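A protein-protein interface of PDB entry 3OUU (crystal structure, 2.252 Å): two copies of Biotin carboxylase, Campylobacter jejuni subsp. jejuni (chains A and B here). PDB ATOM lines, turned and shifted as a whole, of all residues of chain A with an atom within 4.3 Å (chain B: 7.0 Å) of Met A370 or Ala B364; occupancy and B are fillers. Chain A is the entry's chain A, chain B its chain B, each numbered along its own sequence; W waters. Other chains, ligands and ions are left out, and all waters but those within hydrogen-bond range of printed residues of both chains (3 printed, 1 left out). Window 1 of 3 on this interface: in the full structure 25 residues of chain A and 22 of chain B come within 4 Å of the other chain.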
ATOM      1  N   ARG A  23      26.081 -34.488  -8.949  1.00  0.00           N
ATOM      2  CA  ARG A  23      25.560 -33.426  -9.836  1.00  0.00           C
ATOM      3  C   ARG A  23      26.608 -32.442 -10.329  1.00  0.00           C
ATOM      4  O   ARG A  23      26.672 -32.130 -11.515  1.00  0.00           O
ATOM      5  CB  ARG A  23      24.432 -32.646  -9.159  1.00  0.00           C
ATOM      6  CG  ARG A  23      23.199 -33.498  -8.978  1.00  0.00           C
ATOM      7  CD  ARG A  23      22.209 -32.910  -7.997  1.00  0.00           C
ATOM      8  NE  ARG A  23      20.954 -33.624  -8.150  1.00  0.00           N
ATOM      9  CZ  ARG A  23      20.019 -33.727  -7.214  1.00  0.00           C
ATOM     10  NH1 ARG A  23      20.195 -33.164  -6.018  1.00  0.00           N
ATOM     11  NH2 ARG A  23      18.904 -34.394  -7.486  1.00  0.00           N
ATOM     12  N   TYR A 360       6.281 -39.404  -0.780  1.00  0.00           N
ATOM     13  CA  TYR A 360       7.342 -38.431  -0.789  1.00  0.00           C
ATOM     14  C   TYR A 360       7.071 -37.380  -1.866  1.00  0.00           C
ATOM     15  O   TYR A 360       7.138 -37.646  -3.059  1.00  0.00           O
ATOM     16  CB  TYR A 360       8.710 -39.101  -1.010  1.00  0.00           C
ATOM     17  CG  TYR A 360       9.837 -38.101  -0.906  1.00  0.00           C
ATOM     18  CD1 TYR A 360      10.235 -37.616   0.327  1.00  0.00           C
ATOM     19  CD2 TYR A 360      10.458 -37.598  -2.042  1.00  0.00           C
ATOM     20  CE1 TYR A 360      11.239 -36.671   0.435  1.00  0.00           C
ATOM     21  CE2 TYR A 360      11.470 -36.656  -1.945  1.00  0.00           C
ATOM     22  CZ  TYR A 360      11.857 -36.196  -0.701  1.00  0.00           C
ATOM     23  OH  TYR A 360      12.858 -35.260  -0.582  1.00  0.00           O
ATOM     24  N   PRO A 362       8.530 -33.591  -2.405  1.00  0.00           N
ATOM     25  CA  PRO A 362       9.416 -32.535  -1.873  1.00  0.00           C
ATOM     26  C   PRO A 362       8.927 -31.138  -2.217  1.00  0.00           C
ATOM     27  O   PRO A 362       8.196 -30.972  -3.181  1.00  0.00           O
ATOM     28  CB  PRO A 362      10.740 -32.789  -2.584  1.00  0.00           C
ATOM     29  CG  PRO A 362      10.332 -33.408  -3.917  1.00  0.00           C
ATOM     30  CD  PRO A 362       9.079 -34.239  -3.613  1.00  0.00           C
ATOM     31  N   PRO A 363       9.320 -30.128  -1.432  1.00  0.00           N
ATOM     32  CA  PRO A 363       8.941 -28.785  -1.856  1.00  0.00           C
ATOM     33  C   PRO A 363       9.818 -28.340  -3.029  1.00  0.00           C
ATOM     34  O   PRO A 363      10.846 -28.954  -3.319  1.00  0.00           O
ATOM     35  CB  PRO A 363       9.260 -27.940  -0.630  1.00  0.00           C
ATOM     36  CG  PRO A 363      10.349 -28.641   0.019  1.00  0.00           C
ATOM     37  CD  PRO A 363      10.100 -30.107  -0.192  1.00  0.00           C
ATOM     38  N   VAL A 368      14.272 -22.338  -3.643  1.00  0.00           N
ATOM     39  CA  VAL A 368      14.091 -23.437  -2.699  1.00  0.00           C
ATOM     40  C   VAL A 368      14.946 -24.615  -3.178  1.00  0.00           C
ATOM     41  O   VAL A 368      14.880 -24.978  -4.330  1.00  0.00           O
ATOM     42  CB  VAL A 368      12.593 -23.885  -2.600  1.00  0.00           C
ATOM     43  CG1 VAL A 368      12.471 -25.118  -1.706  1.00  0.00           C
ATOM     44  CG2 VAL A 368      11.710 -22.760  -2.037  1.00  0.00           C
ATOM     45  N   ARG A 369      15.780 -25.178  -2.304  1.00  0.00           N
ATOM     46  CA  ARG A 369      16.641 -26.326  -2.644  1.00  0.00           C
ATOM     47  C   ARG A 369      16.351 -27.447  -1.659  1.00  0.00           C
ATOM     48  O   ARG A 369      16.637 -27.324  -0.462  1.00  0.00           O
ATOM     49  CB  ARG A 369      18.119 -25.976  -2.479  1.00  0.00           C
ATOM     50  CG  ARG A 369      18.884 -25.645  -3.733  1.00  0.00           C
ATOM     51  CD  ARG A 369      20.309 -25.156  -3.415  1.00  0.00           C
ATOM     52  NE  ARG A 369      21.271 -26.248  -3.539  1.00  0.00           N
ATOM     53  CZ  ARG A 369      22.593 -26.101  -3.453  1.00  0.00           C
ATOM     54  NH1 ARG A 369      23.112 -24.899  -3.239  1.00  0.00           N
ATOM     55  NH2 ARG A 369      23.396 -27.161  -3.578  1.00  0.00           N
ATOM     56  N   MET A 370      15.768 -28.531  -2.129  1.00  0.00           N
ATOM     57  CA  MET A 370      15.641 -29.694  -1.284  1.00  0.00           C
ATOM     58  C   MET A 370      16.776 -30.570  -1.754  1.00  0.00           C
ATOM     59  O   MET A 370      16.810 -30.967  -2.902  1.00  0.00           O
ATOM     60  CB  MET A 370      14.264 -30.340  -1.435  1.00  0.00           C
ATOM     61  CG  MET A 370      14.031 -31.642  -0.600  1.00  0.00           C
ATOM     62  SD  MET A 370      14.307 -31.498   1.380  1.00  0.00           S
ATOM     63  CE  MET A 370      13.362 -33.119   1.982  1.00  0.00           C
ATOM     64  N   GLU A 371      17.759 -30.757  -0.879  1.00  0.00           N
ATOM     65  CA  GLU A 371      18.931 -31.598  -1.100  1.00  0.00           C
ATOM     66  C   GLU A 371      18.650 -32.959  -0.439  1.00  0.00           C
ATOM     67  O   GLU A 371      18.812 -33.142   0.782  1.00  0.00           O
ATOM     68  CB  GLU A 371      20.167 -30.961  -0.454  1.00  0.00           C
ATOM     69  CG  GLU A 371      20.641 -29.641  -1.084  1.00  0.00           C
ATOM     70  CD  GLU A 371      21.305 -29.847  -2.455  1.00  0.00           C
ATOM     71  OE1 GLU A 371      21.728 -30.984  -2.745  1.00  0.00           O
ATOM     72  OE2 GLU A 371      21.384 -28.878  -3.246  1.00  0.00           O
ATOM     73  N   SER A 372      18.186 -33.904  -1.234  1.00  0.00           N
ATOM     74  CA  SER A 372      17.783 -35.167  -0.662  1.00  0.00           C
ATOM     75  C   SER A 372      17.986 -36.292  -1.632  1.00  0.00           C
ATOM     76  O   SER A 372      17.880 -36.103  -2.840  1.00  0.00           O
ATOM     77  CB  SER A 372      16.313 -35.117  -0.255  1.00  0.00           C
ATOM     78  OG  SER A 372      15.924 -36.371   0.238  1.00  0.00           O
ATOM     79  N   LYS A 390      18.185 -31.950   3.357  1.00  0.00           N
ATOM     80  CA  LYS A 390      18.333 -30.600   3.875  1.00  0.00           C
ATOM     81  C   LYS A 390      17.416 -29.729   3.053  1.00  0.00           C
ATOM     82  O   LYS A 390      17.459 -29.779   1.824  1.00  0.00           O
ATOM     83  CB  LYS A 390      19.775 -30.098   3.708  1.00  0.00           C
ATOM     84  CG  LYS A 390      20.797 -30.819   4.527  1.00  0.00           C
ATOM     85  CD  LYS A 390      22.200 -30.440   4.082  1.00  0.00           C
ATOM     86  CE  LYS A 390      22.661 -31.306   2.920  1.00  0.00           C
ATOM     87  NZ  LYS A 390      24.053 -30.974   2.500  1.00  0.00           N
ATOM     88  N   LEU A 391      16.585 -28.941   3.719  1.00  0.00           N
ATOM     89  CA  LEU A 391      15.747 -27.982   3.023  1.00  0.00           C
ATOM     90  C   LEU A 391      16.412 -26.594   3.139  1.00  0.00           C
ATOM     91  O   LEU A 391      16.645 -26.086   4.240  1.00  0.00           O
ATOM     92  CB  LEU A 391      14.334 -27.981   3.609  1.00  0.00           C
ATOM     93  CG  LEU A 391      13.295 -27.054   2.967  1.00  0.00           C
ATOM     94  CD1 LEU A 391      13.262 -27.281   1.483  1.00  0.00           C
ATOM     95  CD2 LEU A 391      11.895 -27.329   3.591  1.00  0.00           C
ATOM     96  N   LEU A 412       6.354 -29.930   2.130  1.00  0.00           N
ATOM     97  CA  LEU A 412       7.042 -31.203   2.268  1.00  0.00           C
ATOM     98  C   LEU A 412       6.038 -32.257   2.761  1.00  0.00           C
ATOM     99  O   LEU A 412       5.513 -32.145   3.875  1.00  0.00           O
ATOM    100  CB  LEU A 412       8.212 -31.059   3.235  1.00  0.00           C
ATOM    101  CG  LEU A 412       8.934 -32.375   3.525  1.00  0.00           C
ATOM    102  CD1 LEU A 412       9.338 -33.079   2.229  1.00  0.00           C
ATOM    103  CD2 LEU A 412      10.148 -32.128   4.411  1.00  0.00           C
ATOM    104  N   PRO B 362      11.684 -36.016  -9.569  1.00  0.00           N
ATOM    105  CA  PRO B 362      11.973 -34.715 -10.206  1.00  0.00           C
ATOM    106  C   PRO B 362      13.439 -34.337 -10.012  1.00  0.00           C
ATOM    107  O   PRO B 362      14.051 -34.739  -9.019  1.00  0.00           O
ATOM    108  CB  PRO B 362      11.089 -33.750  -9.419  1.00  0.00           C
ATOM    109  CG  PRO B 362      11.101 -34.351  -8.010  1.00  0.00           C
ATOM    110  CD  PRO B 362      11.156 -35.868  -8.200  1.00  0.00           C
ATOM    111  N   PRO B 363      14.025 -33.600 -10.956  1.00  0.00           N
ATOM    112  CA  PRO B 363      15.410 -33.209 -10.663  1.00  0.00           C
ATOM    113  C   PRO B 363      15.478 -32.171  -9.541  1.00  0.00           C
ATOM    114  O   PRO B 363      14.466 -31.573  -9.156  1.00  0.00           O
ATOM    115  CB  PRO B 363      15.902 -32.610 -11.984  1.00  0.00           C
ATOM    116  CG  PRO B 363      14.666 -32.247 -12.744  1.00  0.00           C
ATOM    117  CD  PRO B 363      13.623 -33.265 -12.333  1.00  0.00           C
ATOM    118  N   ALA B 364      16.676 -31.961  -9.015  1.00  0.00           N
ATOM    119  CA  ALA B 364      16.883 -30.946  -8.002  1.00  0.00           C
ATOM    120  C   ALA B 364      18.329 -30.511  -8.100  1.00  0.00           C
ATOM    121  O   ALA B 364      18.994 -30.827  -9.069  1.00  0.00           O
ATOM    122  CB  ALA B 364      16.565 -31.498  -6.629  1.00  0.00           C
ATOM    123  N   GLY B 365      18.807 -29.763  -7.125  1.00  0.00           N
ATOM    124  CA  GLY B 365      20.160 -29.245  -7.177  1.00  0.00           C
ATOM    125  C   GLY B 365      20.242 -27.727  -7.227  1.00  0.00           C
ATOM    126  O   GLY B 365      19.247 -27.023  -7.319  1.00  0.00           O
ATOM    127  N   ARG B 366      21.458 -27.225  -7.167  1.00  0.00           N
ATOM    128  CA  ARG B 366      21.720 -25.798  -7.240  1.00  0.00           C
ATOM    129  C   ARG B 366      21.162 -25.197  -8.542  1.00  0.00           C
ATOM    130  O   ARG B 366      21.489 -25.640  -9.641  1.00  0.00           O
ATOM    131  CB  ARG B 366      23.245 -25.593  -7.144  1.00  0.00           C
ATOM    132  CG  ARG B 366      23.763 -24.164  -7.265  1.00  0.00           C
ATOM    133  CD  ARG B 366      25.303 -24.101  -6.998  1.00  0.00           C
ATOM    134  NE  ARG B 366      25.764 -22.779  -7.367  1.00  0.00           N
ATOM    135  CZ  ARG B 366      26.237 -22.447  -8.559  1.00  0.00           C
ATOM    136  NH1 ARG B 366      26.372 -23.364  -9.513  1.00  0.00           N
ATOM    137  NH2 ARG B 366      26.590 -21.192  -8.785  1.00  0.00           N
ATOM    138  N   ASN B 367      20.336 -24.174  -8.417  1.00  0.00           N
ATOM    139  CA  ASN B 367      19.842 -23.460  -9.590  1.00  0.00           C
ATOM    140  C   ASN B 367      19.086 -24.342 -10.606  1.00  0.00           C
ATOM    141  O   ASN B 367      19.081 -24.039 -11.799  1.00  0.00           O
ATOM    142  CB  ASN B 367      20.991 -22.739 -10.281  1.00  0.00           C
ATOM    143  CG  ASN B 367      21.693 -21.737  -9.351  1.00  0.00           C
ATOM    144  OD1 ASN B 367      21.048 -21.065  -8.552  1.00  0.00           O
ATOM    145  ND2 ASN B 367      23.017 -21.655  -9.451  1.00  0.00           N
ATOM    146  N   VAL B 368      18.483 -25.428 -10.119  1.00  0.00           N
ATOM    147  CA  VAL B 368      17.493 -26.193 -10.858  1.00  0.00           C
ATOM    148  C   VAL B 368      16.098 -25.938 -10.270  1.00  0.00           C
ATOM    149  O   VAL B 368      15.887 -26.024  -9.065  1.00  0.00           O
ATOM    150  CB  VAL B 368      17.802 -27.706 -10.778  1.00  0.00           C
ATOM    151  CG1 VAL B 368      16.759 -28.516 -11.558  1.00  0.00           C
ATOM    152  CG2 VAL B 368      19.206 -27.963 -11.324  1.00  0.00           C
ATOM    153  N   ARG B 369      15.136 -25.625 -11.125  1.00  0.00           N
ATOM    154  CA  ARG B 369      13.775 -25.298 -10.686  1.00  0.00           C
ATOM    155  C   ARG B 369      12.790 -26.153 -11.482  1.00  0.00           C
ATOM    156  O   ARG B 369      12.573 -25.913 -12.661  1.00  0.00           O
ATOM    157  CB  ARG B 369      13.542 -23.822 -10.983  1.00  0.00           C
ATOM    158  CG  ARG B 369      12.493 -23.122 -10.184  1.00  0.00           C
ATOM    159  CD  ARG B 369      12.438 -21.655 -10.595  1.00  0.00           C
ATOM    160  NE  ARG B 369      11.084 -21.156 -10.473  1.00  0.00           N
ATOM    161  CZ  ARG B 369      10.709 -19.881 -10.585  1.00  0.00           C
ATOM    162  NH1 ARG B 369      11.591 -18.916 -10.812  1.00  0.00           N
ATOM    163  NH2 ARG B 369       9.425 -19.561 -10.450  1.00  0.00           N
ATOM    164  N   MET B 370      12.235 -27.191 -10.879  1.00  0.00           N
ATOM    165  CA  MET B 370      11.233 -27.994 -11.592  1.00  0.00           C
ATOM    166  C   MET B 370       9.839 -27.483 -11.219  1.00  0.00           C
ATOM    167  O   MET B 370       9.382 -27.685 -10.097  1.00  0.00           O
ATOM    168  CB  MET B 370      11.376 -29.475 -11.254  1.00  0.00           C
ATOM    169  CG  MET B 370      10.273 -30.362 -11.837  1.00  0.00           C
ATOM    170  SD  MET B 370      10.230 -30.428 -13.810  1.00  0.00           S
ATOM    171  CE  MET B 370       8.825 -31.765 -14.044  1.00  0.00           C
ATOM    172  N   LEU B 391      10.979 -27.517 -16.687  1.00  0.00           N
ATOM    173  CA  LEU B 391      12.271 -27.691 -16.082  1.00  0.00           C
ATOM    174  C   LEU B 391      13.117 -26.438 -16.408  1.00  0.00           C
ATOM    175  O   LEU B 391      13.413 -26.139 -17.571  1.00  0.00           O
ATOM    176  CB  LEU B 391      12.909 -28.982 -16.609  1.00  0.00           C
ATOM    177  CG  LEU B 391      14.315 -29.349 -16.098  1.00  0.00           C
ATOM    178  CD1 LEU B 391      14.462 -29.119 -14.598  1.00  0.00           C
ATOM    179  CD2 LEU B 391      14.684 -30.800 -16.446  1.00  0.00           C
ATOM    180  N   LYS B 404      24.099 -27.945 -17.392  1.00  0.00           N
ATOM    181  CA  LYS B 404      23.267 -28.102 -16.201  1.00  0.00           C
ATOM    182  C   LYS B 404      21.882 -28.675 -16.573  1.00  0.00           C
ATOM    183  O   LYS B 404      21.348 -29.520 -15.859  1.00  0.00           O
ATOM    184  CB  LYS B 404      23.159 -26.776 -15.409  1.00  0.00           C
ATOM    185  CG  LYS B 404      22.229 -26.853 -14.215  1.00  0.00           C
ATOM    186  CD  LYS B 404      22.196 -25.580 -13.394  1.00  0.00           C
ATOM    187  CE  LYS B 404      23.440 -25.438 -12.525  1.00  0.00           C
ATOM    188  NZ  LYS B 404      23.505 -26.517 -11.508  1.00  0.00           N
ATOM    189  N   VAL B 407      22.148 -32.607 -17.248  1.00  0.00           N
ATOM    190  CA  VAL B 407      22.165 -33.345 -15.992  1.00  0.00           C
ATOM    191  C   VAL B 407      20.791 -33.398 -15.339  1.00  0.00           C
ATOM    192  O   VAL B 407      20.373 -34.480 -14.890  1.00  0.00           O
ATOM    193  CB  VAL B 407      23.196 -32.789 -14.975  1.00  0.00           C
ATOM    194  CG1 VAL B 407      23.000 -33.462 -13.596  1.00  0.00           C
ATOM    195  CG2 VAL B 407      24.617 -32.985 -15.498  1.00  0.00           C
ATOM    196  N   ALA B 408      20.087 -32.261 -15.279  1.00  0.00           N
ATOM    197  CA  ALA B 408      18.740 -32.266 -14.694  1.00  0.00           C
ATOM    198  C   ALA B 408      17.751 -33.193 -15.445  1.00  0.00           C
ATOM    199  O   ALA B 408      16.965 -33.925 -14.816  1.00  0.00           O
ATOM    200  CB  ALA B 408      18.171 -30.827 -14.560  1.00  0.00           C
ATOM    201  N   GLU B 411      18.117 -36.675 -14.736  1.00  0.00           N
ATOM    202  CA  GLU B 411      17.701 -37.051 -13.383  1.00  0.00           C
ATOM    203  C   GLU B 411      16.195 -37.143 -13.222  1.00  0.00           C
ATOM    204  O   GLU B 411      15.705 -37.720 -12.248  1.00  0.00           O
ATOM    205  CB  GLU B 411      18.315 -36.138 -12.324  1.00  0.00           C
ATOM    206  CG  GLU B 411      19.779 -36.430 -12.157  1.00  0.00           C
ATOM    207  CD  GLU B 411      20.531 -35.442 -11.259  1.00  0.00           C
ATOM    208  OE1 GLU B 411      19.902 -34.550 -10.613  1.00  0.00           O
ATOM    209  OE2 GLU B 411      21.782 -35.585 -11.224  1.00  0.00           O
HETATM  210  O   HOH W   1      16.694 -36.314  -8.810  1.00  0.00           O
HETATM  211  O   HOH W   2      18.283 -29.675  -4.583  1.00  0.00           O
HETATM  212  O   HOH W   3      16.321 -24.249  -6.673  1.00  0.00           O
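NE of Arg A23 touches O of Ala B364, 3.5 Å away. Arg A23 touches Gly B365. CG of Arg A369 touches O of Gly B365, at 3.9 Å. Arg A369 touches Arg B366. Met A370 touches Ala B364.
Among the printed residues, Asp or Glu carboxylates within 4 Å of a Lys or Arg side-chain nitrogen of the other chain: Arg A23 with Glu B411.
NE of Arg A23 lies within salt-bridge range of OE1 of Glu B411, 2.8 Å away.
Positions printed for both chains: 362, 363, 368, 369, 370 and 391.
Water W2 lies within hydrogen-bond range of the backbone carbonyl oxygen of Met A370, the backbone NH of Gly B365 and the side-chain carboxylate of Glu A371. Water W3 lies within hydrogen-bond range of the backbone carbonyl oxygen (O) of Val A368 and the backbone carbonyl oxygen (O) of Val B368. Water W1 lies within hydrogen-bond range of O of Pro B362 (3.1 Å) and NH2 of Arg A23 (3.2 Å).
Printed residues of chain B within 4 Å of Arg A23: Ala B364, Gly B365 and Glu B411. Val A368 touches none of the printed residues of chain B. Of the printed residues of chain B, Arg A369 touches Gly B365 and Arg B366. Met A370 touches just one residue of chain B: Ala B364. Ala B364 touches two residues of chain A. Printed residues of chain A within 4 Å of Gly B365: Arg A23 (3.8 Å) and Arg A369 (3.9 Å). Of the printed residues of chain A, Arg B366 touches Arg A369 (3.8 Å). Asn B367 touches none of the printed residues of chain A. The nearest residue of chain B that does not touch Met A370 is Gly B365 (4.8 Å). The nearest printed residue of chain A that does not touch Ala B364 is Glu A371 (5.9 Å).
The guanidinium group (NE) of Arg A369 lies within salt-bridge range of the side-chain carboxylate (OE2) of Glu A371, at 2.6 Å. O of Arg B366 is in hydrogen-bond range of NZ of Lys B404 (2.9 Å).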
